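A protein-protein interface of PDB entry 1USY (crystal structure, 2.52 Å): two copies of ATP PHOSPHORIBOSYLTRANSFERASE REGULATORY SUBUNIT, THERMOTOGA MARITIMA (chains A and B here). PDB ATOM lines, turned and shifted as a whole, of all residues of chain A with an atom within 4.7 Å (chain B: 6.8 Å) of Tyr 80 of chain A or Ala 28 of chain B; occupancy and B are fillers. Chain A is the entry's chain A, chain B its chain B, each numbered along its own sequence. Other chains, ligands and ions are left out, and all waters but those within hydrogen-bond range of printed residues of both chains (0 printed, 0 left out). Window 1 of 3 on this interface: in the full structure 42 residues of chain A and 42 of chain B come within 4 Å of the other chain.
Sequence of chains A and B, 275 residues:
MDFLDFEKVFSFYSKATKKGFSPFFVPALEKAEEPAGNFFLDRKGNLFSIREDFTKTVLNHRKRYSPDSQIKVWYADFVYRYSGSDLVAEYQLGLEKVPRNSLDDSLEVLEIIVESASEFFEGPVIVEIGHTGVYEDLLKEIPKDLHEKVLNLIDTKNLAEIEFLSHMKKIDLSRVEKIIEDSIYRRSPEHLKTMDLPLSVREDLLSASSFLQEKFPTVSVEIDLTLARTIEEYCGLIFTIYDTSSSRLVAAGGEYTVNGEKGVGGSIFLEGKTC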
ATOM      1  N   ALA A  28     -25.870   2.204  -6.388  1.00  0.00           N
ATOM      2  CA  ALA A  28     -26.228   3.565  -5.983  1.00  0.00           C
ATOM      3  C   ALA A  28     -26.704   4.489  -7.124  1.00  0.00           C
ATOM      4  O   ALA A  28     -27.487   5.423  -6.893  1.00  0.00           O
ATOM      5  CB  ALA A  28     -25.002   4.210  -5.305  1.00  0.00           C
ATOM      6  N   ILE A  50     -29.272   9.250  -8.364  1.00  0.00           N
ATOM      7  CA  ILE A  50     -28.643   8.539  -7.250  1.00  0.00           C
ATOM      8  C   ILE A  50     -29.662   8.103  -6.199  1.00  0.00           C
ATOM      9  O   ILE A  50     -30.679   8.756  -6.029  1.00  0.00           O
ATOM     10  CB  ILE A  50     -27.499   9.379  -6.627  1.00  0.00           C
ATOM     11  CG1 ILE A  50     -26.509   8.467  -5.870  1.00  0.00           C
ATOM     12  CG2 ILE A  50     -28.060  10.494  -5.734  1.00  0.00           C
ATOM     13  CD1 ILE A  50     -25.129   9.105  -5.657  1.00  0.00           C
ATOM     14  N   ARG A  51     -29.407   6.981  -5.524  1.00  0.00           N
ATOM     15  CA  ARG A  51     -30.287   6.514  -4.454  1.00  0.00           C
ATOM     16  C   ARG A  51     -30.515   7.590  -3.401  1.00  0.00           C
ATOM     17  O   ARG A  51     -29.644   7.854  -2.580  1.00  0.00           O
ATOM     18  CB  ARG A  51     -29.696   5.302  -3.757  1.00  0.00           C
ATOM     19  CG  ARG A  51     -30.662   4.623  -2.805  1.00  0.00           C
ATOM     20  CD  ARG A  51     -29.993   3.569  -1.977  1.00  0.00           C
ATOM     21  NE  ARG A  51     -29.404   2.589  -2.869  1.00  0.00           N
ATOM     22  CZ  ARG A  51     -28.151   2.177  -2.879  1.00  0.00           C
ATOM     23  NH1 ARG A  51     -27.239   2.613  -2.026  1.00  0.00           N
ATOM     24  NH2 ARG A  51     -27.825   1.289  -3.791  1.00  0.00           N
ATOM     25  N   GLU A  52     -31.695   8.201  -3.416  1.00  0.00           N
ATOM     26  CA  GLU A  52     -32.013   9.223  -2.421  1.00  0.00           C
ATOM     27  C   GLU A  52     -32.998   8.706  -1.394  1.00  0.00           C
ATOM     28  O   GLU A  52     -33.095   9.226  -0.294  1.00  0.00           O
ATOM     29  CB  GLU A  52     -32.474  10.525  -3.100  1.00  0.00           C
ATOM     30  CG  GLU A  52     -31.316  11.178  -3.851  1.00  0.00           C
ATOM     31  CD  GLU A  52     -31.648  12.478  -4.569  1.00  0.00           C
ATOM     32  OE1 GLU A  52     -32.323  12.442  -5.622  1.00  0.00           O
ATOM     33  OE2 GLU A  52     -31.193  13.545  -4.096  1.00  0.00           O
ATOM     34  N   PHE A  78     -25.668   2.736   1.428  1.00  0.00           N
ATOM     35  CA  PHE A  78     -25.622   4.179   1.553  1.00  0.00           C
ATOM     36  C   PHE A  78     -26.811   4.789   0.865  1.00  0.00           C
ATOM     37  O   PHE A  78     -27.186   4.331  -0.191  1.00  0.00           O
ATOM     38  CB  PHE A  78     -24.342   4.706   0.943  1.00  0.00           C
ATOM     39  CG  PHE A  78     -23.180   4.584   1.841  1.00  0.00           C
ATOM     40  CD1 PHE A  78     -22.209   3.600   1.618  1.00  0.00           C
ATOM     41  CD2 PHE A  78     -23.065   5.437   2.940  1.00  0.00           C
ATOM     42  CE1 PHE A  78     -21.092   3.486   2.467  1.00  0.00           C
ATOM     43  CE2 PHE A  78     -21.978   5.353   3.810  1.00  0.00           C
ATOM     44  CZ  PHE A  78     -20.968   4.373   3.583  1.00  0.00           C
ATOM     45  N   VAL A  79     -27.395   5.823   1.464  1.00  0.00           N
ATOM     46  CA  VAL A  79     -28.400   6.648   0.802  1.00  0.00           C
ATOM     47  C   VAL A  79     -27.773   8.037   0.697  1.00  0.00           C
ATOM     48  O   VAL A  79     -27.072   8.470   1.624  1.00  0.00           O
ATOM     49  CB  VAL A  79     -29.719   6.683   1.621  1.00  0.00           C
ATOM     50  CG1 VAL A  79     -30.728   7.668   1.035  1.00  0.00           C
ATOM     51  CG2 VAL A  79     -30.346   5.311   1.704  1.00  0.00           C
ATOM     52  N   TYR A  80     -27.989   8.714  -0.432  1.00  0.00           N
ATOM     53  CA  TYR A  80     -27.282   9.968  -0.745  1.00  0.00           C
ATOM     54  C   TYR A  80     -28.215  11.187  -0.638  1.00  0.00           C
ATOM     55  O   TYR A  80     -29.437  11.048  -0.730  1.00  0.00           O
ATOM     56  CB  TYR A  80     -26.586   9.902  -2.137  1.00  0.00           C
ATOM     57  CG  TYR A  80     -25.585   8.784  -2.250  1.00  0.00           C
ATOM     58  CD1 TYR A  80     -26.024   7.464  -2.411  1.00  0.00           C
ATOM     59  CD2 TYR A  80     -24.189   9.021  -2.178  1.00  0.00           C
ATOM     60  CE1 TYR A  80     -25.129   6.416  -2.512  1.00  0.00           C
ATOM     61  CE2 TYR A  80     -23.260   7.938  -2.272  1.00  0.00           C
ATOM     62  CZ  TYR A  80     -23.753   6.653  -2.457  1.00  0.00           C
ATOM     63  OH  TYR A  80     -22.911   5.573  -2.556  1.00  0.00           O
ATOM     64  N   ARG A  81     -27.648  12.367  -0.388  1.00  0.00           N
ATOM     65  CA  ARG A  81     -28.438  13.599  -0.297  1.00  0.00           C
ATOM     66  C   ARG A  81     -27.498  14.776  -0.370  1.00  0.00           C
ATOM     67  O   ARG A  81     -26.287  14.610  -0.242  1.00  0.00           O
ATOM     68  CB  ARG A  81     -29.305  13.643   0.981  1.00  0.00           C
ATOM     69  CG  ARG A  81     -28.590  14.261   2.169  1.00  0.00           C
ATOM     70  CD  ARG A  81     -28.925  13.674   3.551  1.00  0.00           C
ATOM     71  NE  ARG A  81     -28.388  14.533   4.606  1.00  0.00           N
ATOM     72  CZ  ARG A  81     -27.570  14.131   5.590  1.00  0.00           C
ATOM     73  NH1 ARG A  81     -27.139  15.021   6.495  1.00  0.00           N
ATOM     74  NH2 ARG A  81     -27.180  12.850   5.682  1.00  0.00           N
ATOM     75  N   LEU A  87     -22.335  16.515  -1.721  1.00  0.00           N
ATOM     76  CA  LEU A  87     -23.002  15.204  -1.684  1.00  0.00           C
ATOM     77  C   LEU A  87     -22.573  14.496  -0.427  1.00  0.00           C
ATOM     78  O   LEU A  87     -21.397  14.383  -0.184  1.00  0.00           O
ATOM     79  CB  LEU A  87     -22.629  14.332  -2.902  1.00  0.00           C
ATOM     80  CG  LEU A  87     -23.659  13.572  -3.768  1.00  0.00           C
ATOM     81  CD1 LEU A  87     -23.021  12.290  -4.145  1.00  0.00           C
ATOM     82  CD2 LEU A  87     -25.064  13.333  -3.181  1.00  0.00           C
ATOM     83  N   VAL A  88     -23.535  14.057   0.360  1.00  0.00           N
ATOM     84  CA  VAL A  88     -23.276  13.278   1.565  1.00  0.00           C
ATOM     85  C   VAL A  88     -24.066  11.986   1.449  1.00  0.00           C
ATOM     86  O   VAL A  88     -24.915  11.838   0.586  1.00  0.00           O
ATOM     87  CB  VAL A  88     -23.647  14.048   2.929  1.00  0.00           C
ATOM     88  CG1 VAL A  88     -22.793  15.274   3.104  1.00  0.00           C
ATOM     89  CG2 VAL A  88     -25.103  14.438   2.989  1.00  0.00           C
ATOM     90  N   ALA A  89     -23.805  11.078   2.365  1.00  0.00           N
ATOM     91  CA  ALA A  89     -24.260   9.726   2.252  1.00  0.00           C
ATOM     92  C   ALA A  89     -24.436   9.252   3.669  1.00  0.00           C
ATOM     93  O   ALA A  89     -23.602   9.555   4.504  1.00  0.00           O
ATOM     94  CB  ALA A  89     -23.190   8.905   1.544  1.00  0.00           C
ATOM     95  N   CYS A 275     -19.702  12.518   0.425  1.00  0.00           N
ATOM     96  CA  CYS A 275     -19.794  12.186  -0.996  1.00  0.00           C
ATOM     97  C   CYS A 275     -21.002  11.299  -1.272  1.00  0.00           C
ATOM     98  O   CYS A 275     -20.911  10.126  -1.608  1.00  0.00           O
ATOM     99  CB  CYS A 275     -18.502  11.566  -1.512  1.00  0.00           C
ATOM    100  SG  CYS A 275     -17.204  12.800  -1.719  1.00  0.00           S
ATOM    101  OXT CYS A 275     -22.158  11.771  -1.155  1.00  0.00           O
ATOM    102  N   VAL B  26     -17.429   2.559   2.153  1.00  0.00           N
ATOM    103  CA  VAL B  26     -17.430   3.941   1.692  1.00  0.00           C
ATOM    104  C   VAL B  26     -18.412   4.193   0.546  1.00  0.00           C
ATOM    105  O   VAL B  26     -18.801   3.280  -0.159  1.00  0.00           O
ATOM    106  CB  VAL B  26     -16.023   4.414   1.217  1.00  0.00           C
ATOM    107  CG1 VAL B  26     -15.038   4.336   2.325  1.00  0.00           C
ATOM    108  CG2 VAL B  26     -15.541   3.607   0.017  1.00  0.00           C
ATOM    109  N   PRO B  27     -18.837   5.449   0.388  1.00  0.00           N
ATOM    110  CA  PRO B  27     -19.676   5.853  -0.736  1.00  0.00           C
ATOM    111  C   PRO B  27     -19.108   5.503  -2.069  1.00  0.00           C
ATOM    112  O   PRO B  27     -17.923   5.675  -2.264  1.00  0.00           O
ATOM    113  CB  PRO B  27     -19.697   7.375  -0.605  1.00  0.00           C
ATOM    114  CG  PRO B  27     -19.597   7.605   0.837  1.00  0.00           C
ATOM    115  CD  PRO B  27     -18.621   6.556   1.334  1.00  0.00           C
ATOM    116  N   ALA B  28     -19.961   5.044  -2.984  1.00  0.00           N
ATOM    117  CA  ALA B  28     -19.595   4.802  -4.376  1.00  0.00           C
ATOM    118  C   ALA B  28     -19.030   6.058  -5.095  1.00  0.00           C
ATOM    119  O   ALA B  28     -18.075   5.968  -5.867  1.00  0.00           O
ATOM    120  CB  ALA B  28     -20.813   4.266  -5.122  1.00  0.00           C
ATOM    121  N   LEU B  29     -19.639   7.205  -4.854  1.00  0.00           N
ATOM    122  CA  LEU B  29     -19.196   8.452  -5.456  1.00  0.00           C
ATOM    123  C   LEU B  29     -18.203   9.150  -4.530  1.00  0.00           C
ATOM    124  O   LEU B  29     -18.370   9.121  -3.320  1.00  0.00           O
ATOM    125  CB  LEU B  29     -20.400   9.366  -5.732  1.00  0.00           C
ATOM    126  CG  LEU B  29     -21.056   9.132  -7.089  1.00  0.00           C
ATOM    127  CD1 LEU B  29     -22.162  10.130  -7.340  1.00  0.00           C
ATOM    128  CD2 LEU B  29     -20.041   9.202  -8.214  1.00  0.00           C
ATOM    129  N   GLU B  30     -17.171   9.756  -5.106  1.00  0.00           N
ATOM    130  CA  GLU B  30     -16.186  10.532  -4.359  1.00  0.00           C
ATOM    131  C   GLU B  30     -15.803  11.789  -5.157  1.00  0.00           C
ATOM    132  O   GLU B  30     -15.383  11.697  -6.309  1.00  0.00           O
ATOM    133  CB  GLU B  30     -14.954   9.677  -4.060  1.00  0.00           C
ATOM    134  CG  GLU B  30     -15.063   8.895  -2.753  1.00  0.00           C
ATOM    135  CD  GLU B  30     -13.965   7.860  -2.558  1.00  0.00           C
ATOM    136  OE1 GLU B  30     -12.915   7.953  -3.232  1.00  0.00           O
ATOM    137  OE2 GLU B  30     -14.159   6.948  -1.726  1.00  0.00           O
ATOM    138  N   SER B  49     -15.572  10.895  -9.157  1.00  0.00           N
ATOM    139  CA  SER B  49     -15.152   9.590  -9.629  1.00  0.00           C
ATOM    140  C   SER B  49     -16.041   8.591  -8.963  1.00  0.00           C
ATOM    141  O   SER B  49     -16.551   8.834  -7.865  1.00  0.00           O
ATOM    142  CB  SER B  49     -13.697   9.265  -9.284  1.00  0.00           C
ATOM    143  OG  SER B  49     -13.281   9.980  -8.142  1.00  0.00           O
ATOM    144  N   ILE B  50     -16.236   7.474  -9.661  1.00  0.00           N
ATOM    145  CA  ILE B  50     -17.029   6.357  -9.175  1.00  0.00           C
ATOM    146  C   ILE B  50     -16.088   5.189  -8.982  1.00  0.00           C
ATOM    147  O   ILE B  50     -15.134   5.026  -9.745  1.00  0.00           O
ATOM    148  CB  ILE B  50     -18.163   6.020 -10.145  1.00  0.00           C
ATOM    149  CG1 ILE B  50     -19.234   5.200  -9.430  1.00  0.00           C
ATOM    150  CG2 ILE B  50     -17.630   5.271 -11.346  1.00  0.00           C
ATOM    151  CD1 ILE B  50     -20.542   5.054 -10.179  1.00  0.00           C
ATOM    152  N   ARG B  51     -16.354   4.396  -7.943  1.00  0.00           N
ATOM    153  CA  ARG B  51     -15.430   3.377  -7.470  1.00  0.00           C
ATOM    154  C   ARG B  51     -15.212   2.329  -8.566  1.00  0.00           C
ATOM    155  O   ARG B  51     -16.128   1.601  -8.929  1.00  0.00           O
ATOM    156  CB  ARG B  51     -15.977   2.771  -6.175  1.00  0.00           C
ATOM    157  CG  ARG B  51     -15.214   1.592  -5.609  1.00  0.00           C
ATOM    158  CD  ARG B  51     -16.010   0.737  -4.616  1.00  0.00           C
ATOM    159  NE  ARG B  51     -16.700   1.556  -3.626  1.00  0.00           N
ATOM    160  CZ  ARG B  51     -17.971   1.404  -3.272  1.00  0.00           C
ATOM    161  NH1 ARG B  51     -18.711   0.444  -3.793  1.00  0.00           N
ATOM    162  NH2 ARG B  51     -18.517   2.209  -2.382  1.00  0.00           N
ATOM    163  N   GLU B  52     -13.995   2.293  -9.103  1.00  0.00           N
ATOM    164  CA  GLU B  52     -13.634   1.440 -10.231  1.00  0.00           C
ATOM    165  C   GLU B  52     -12.621   0.417  -9.792  1.00  0.00           C
ATOM    166  O   GLU B  52     -12.431  -0.586 -10.458  1.00  0.00           O
ATOM    167  CB  GLU B  52     -13.033   2.266 -11.358  1.00  0.00           C
ATOM    168  CG  GLU B  52     -14.066   3.030 -12.153  1.00  0.00           C
ATOM    169  CD  GLU B  52     -13.492   3.750 -13.364  1.00  0.00           C
ATOM    170  OE1 GLU B  52     -13.151   4.956 -13.264  1.00  0.00           O
ATOM    171  OE2 GLU B  52     -13.405   3.118 -14.434  1.00  0.00           O
ATOM    172  N   THR B  57      -9.209   2.775  -4.339  1.00  0.00           N
ATOM    173  CA  THR B  57     -10.018   3.426  -3.313  1.00  0.00           C
ATOM    174  C   THR B  57      -9.461   3.298  -1.897  1.00  0.00           C
ATOM    175  O   THR B  57      -9.402   4.266  -1.172  1.00  0.00           O
ATOM    176  CB  THR B  57     -11.442   2.860  -3.355  1.00  0.00           C
ATOM    177  OG1 THR B  57     -12.127   3.422  -4.478  1.00  0.00           O
ATOM    178  CG2 THR B  57     -12.240   3.326  -2.142  1.00  0.00           C
ATOM    179  N   ASP B  77     -18.917  -4.481  -1.610  1.00  0.00           N
ATOM    180  CA  ASP B  77     -19.712  -3.498  -2.315  1.00  0.00           C
ATOM    181  C   ASP B  77     -19.603  -3.623  -3.844  1.00  0.00           C
ATOM    182  O   ASP B  77     -18.885  -4.473  -4.402  1.00  0.00           O
ATOM    183  CB  ASP B  77     -19.288  -2.102  -1.878  1.00  0.00           C
ATOM    184  CG  ASP B  77     -20.472  -1.126  -1.744  1.00  0.00           C
ATOM    185  OD1 ASP B  77     -20.352  -0.224  -0.901  1.00  0.00           O
ATOM    186  OD2 ASP B  77     -21.542  -1.154  -2.409  1.00  0.00           O
ATOM    187  N   PHE B  78     -20.329  -2.754  -4.521  1.00  0.00           N
ATOM    188  CA  PHE B  78     -20.289  -2.699  -5.942  1.00  0.00           C
ATOM    189  C   PHE B  78     -19.020  -2.017  -6.396  1.00  0.00           C
ATOM    190  O   PHE B  78     -18.568  -1.086  -5.742  1.00  0.00           O
ATOM    191  CB  PHE B  78     -21.518  -1.979  -6.438  1.00  0.00           C
ATOM    192  CG  PHE B  78     -22.767  -2.793  -6.306  1.00  0.00           C
ATOM    193  CD1 PHE B  78     -23.719  -2.483  -5.359  1.00  0.00           C
ATOM    194  CD2 PHE B  78     -22.965  -3.910  -7.110  1.00  0.00           C
ATOM    195  CE1 PHE B  78     -24.879  -3.283  -5.240  1.00  0.00           C
ATOM    196  CE2 PHE B  78     -24.120  -4.694  -7.001  1.00  0.00           C
ATOM    197  CZ  PHE B  78     -25.065  -4.391  -6.079  1.00  0.00           C
ATOM    198  N   TYR B  80     -17.760  -0.447 -10.114  1.00  0.00           N
ATOM    199  CA  TYR B  80     -18.495  -0.066 -11.323  1.00  0.00           C
ATOM    200  C   TYR B  80     -17.558  -0.060 -12.485  1.00  0.00           C
ATOM    201  O   TYR B  80     -16.362   0.081 -12.300  1.00  0.00           O
ATOM    202  CB  TYR B  80     -19.113   1.327 -11.179  1.00  0.00           C
ATOM    203  CG  TYR B  80     -20.138   1.429 -10.063  1.00  0.00           C
ATOM    204  CD1 TYR B  80     -19.770   1.330  -8.719  1.00  0.00           C
ATOM    205  CD2 TYR B  80     -21.479   1.641 -10.358  1.00  0.00           C
ATOM    206  CE1 TYR B  80     -20.731   1.433  -7.713  1.00  0.00           C
ATOM    207  CE2 TYR B  80     -22.422   1.738  -9.365  1.00  0.00           C
ATOM    208  CZ  TYR B  80     -22.052   1.633  -8.044  1.00  0.00           C
ATOM    209  OH  TYR B  80     -23.042   1.736  -7.088  1.00  0.00           O
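Ala 28 of chain A touches Tyr 80 of chain B, and with the chains exchanged Tyr 80 of chain A touches Ala 28 of chain B. Positions printed for both chains: 28, 50, 51, 52, 78 and 80.
Ile 50 of chain A touches Leu 29 of chain B. Val 26 of chain B touches Phe 78 of chain A (C to CE1, 3.4 Å). Phe 78 of chain A touches Pro 27 of chain B. Pro 27 of chain B touches Tyr 80 of chain A. Leu 29 of chain B touches Leu 87 of chain A. Ala 89 of chain A touches Pro 27 of chain B (CB to CG, 3.9 Å). CB of Pro 27 of chain B touches O of Cys 275 of chain A, 3.2 Å away. Glu 30 of chain B touches Cys 275 of chain A (CA to SG, 3.6 Å).
Hydrophobic or aromatic side chains of chain B that line the printed part of chain A: Pro 27, Ala 28, Leu 29 and Tyr 80. Hydrophobic or aromatic side chains of chain A within 4 Å of the printed part of chain B: Ala 28, Ile 50, Phe 78, Tyr 80, Leu 87 and Ala 89. Among the printed residues, no Asp or Glu carboxylate lies within 4 Å of a Lys or Arg side-chain nitrogen of the other chain.
The backbone NH (N) of Ala 28 of chain A lies within hydrogen-bond range of the side-chain hydroxyl (OH) of Tyr 80 of chain B (3.0 Å). The backbone NH (N) of Ala 28 of chain B is in hydrogen-bond range of the side-chain hydroxyl (OH) of Tyr 80 of chain A, at 3.0 Å. O of Cys 275 of chain A lies close to O of Leu 29 of chain B, 3.2 Å away.
O of Arg 51 of chain A lies within hydrogen-bond range of N of Tyr 80 of chain A (2.8 Å). N of Cys 275 of chain A sits at hydrogen-bond distance from O of Leu 87 of chain A, 2.6 Å away. The backbone NH (N) of Val 88 of chain A lies within hydrogen-bond range of the chain-end carboxylate (OXT) of Cys 275 of chain A, at 3.1 Å. NH2 of Arg 51 of chain B lies within hydrogen-bond range of O of Val 26 of chain B (2.5 Å). The backbone carbonyl oxygen (O) of Ala 28 of chain B sits at hydrogen-bond distance from the backbone NH (N) of Arg 51 of chain B (3.1 Å). N of Tyr 80 of chain B lies within hydrogen-bond range of O of Arg 51 of chain B, at 2.9 Å.
Printed residues of chain B within 4 Å of Ala 28 of chain A: Tyr 80. Tyr 80 of chain A touches just these residues of chain B: Pro 27 (3.7 Å) and Ala 28 (3.0 Å). Of the printed residues of chain A, Pro 27 of chain B touches Phe 78 (3.6 Å), Tyr 80 (3.7 Å), Ala 89 (3.9 Å) and Cys 275 (3.2 Å). Ala 28 of chain B touches one residue of chain A. Of the printed residues of chain A, Leu 29 of chain B touches Ile 50 (3.6 Å), Leu 87 (3.95 Å) and Cys 275 (3.0 Å). Of the printed residues of chain A, Glu 30 of chain B touches Cys 275. Asp 77 of chain B touches none of the printed residues of chain A. The nearest residue of chain A that does not touch Ala 28 of chain B is Ala 28 of chain A (4.2 Å).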
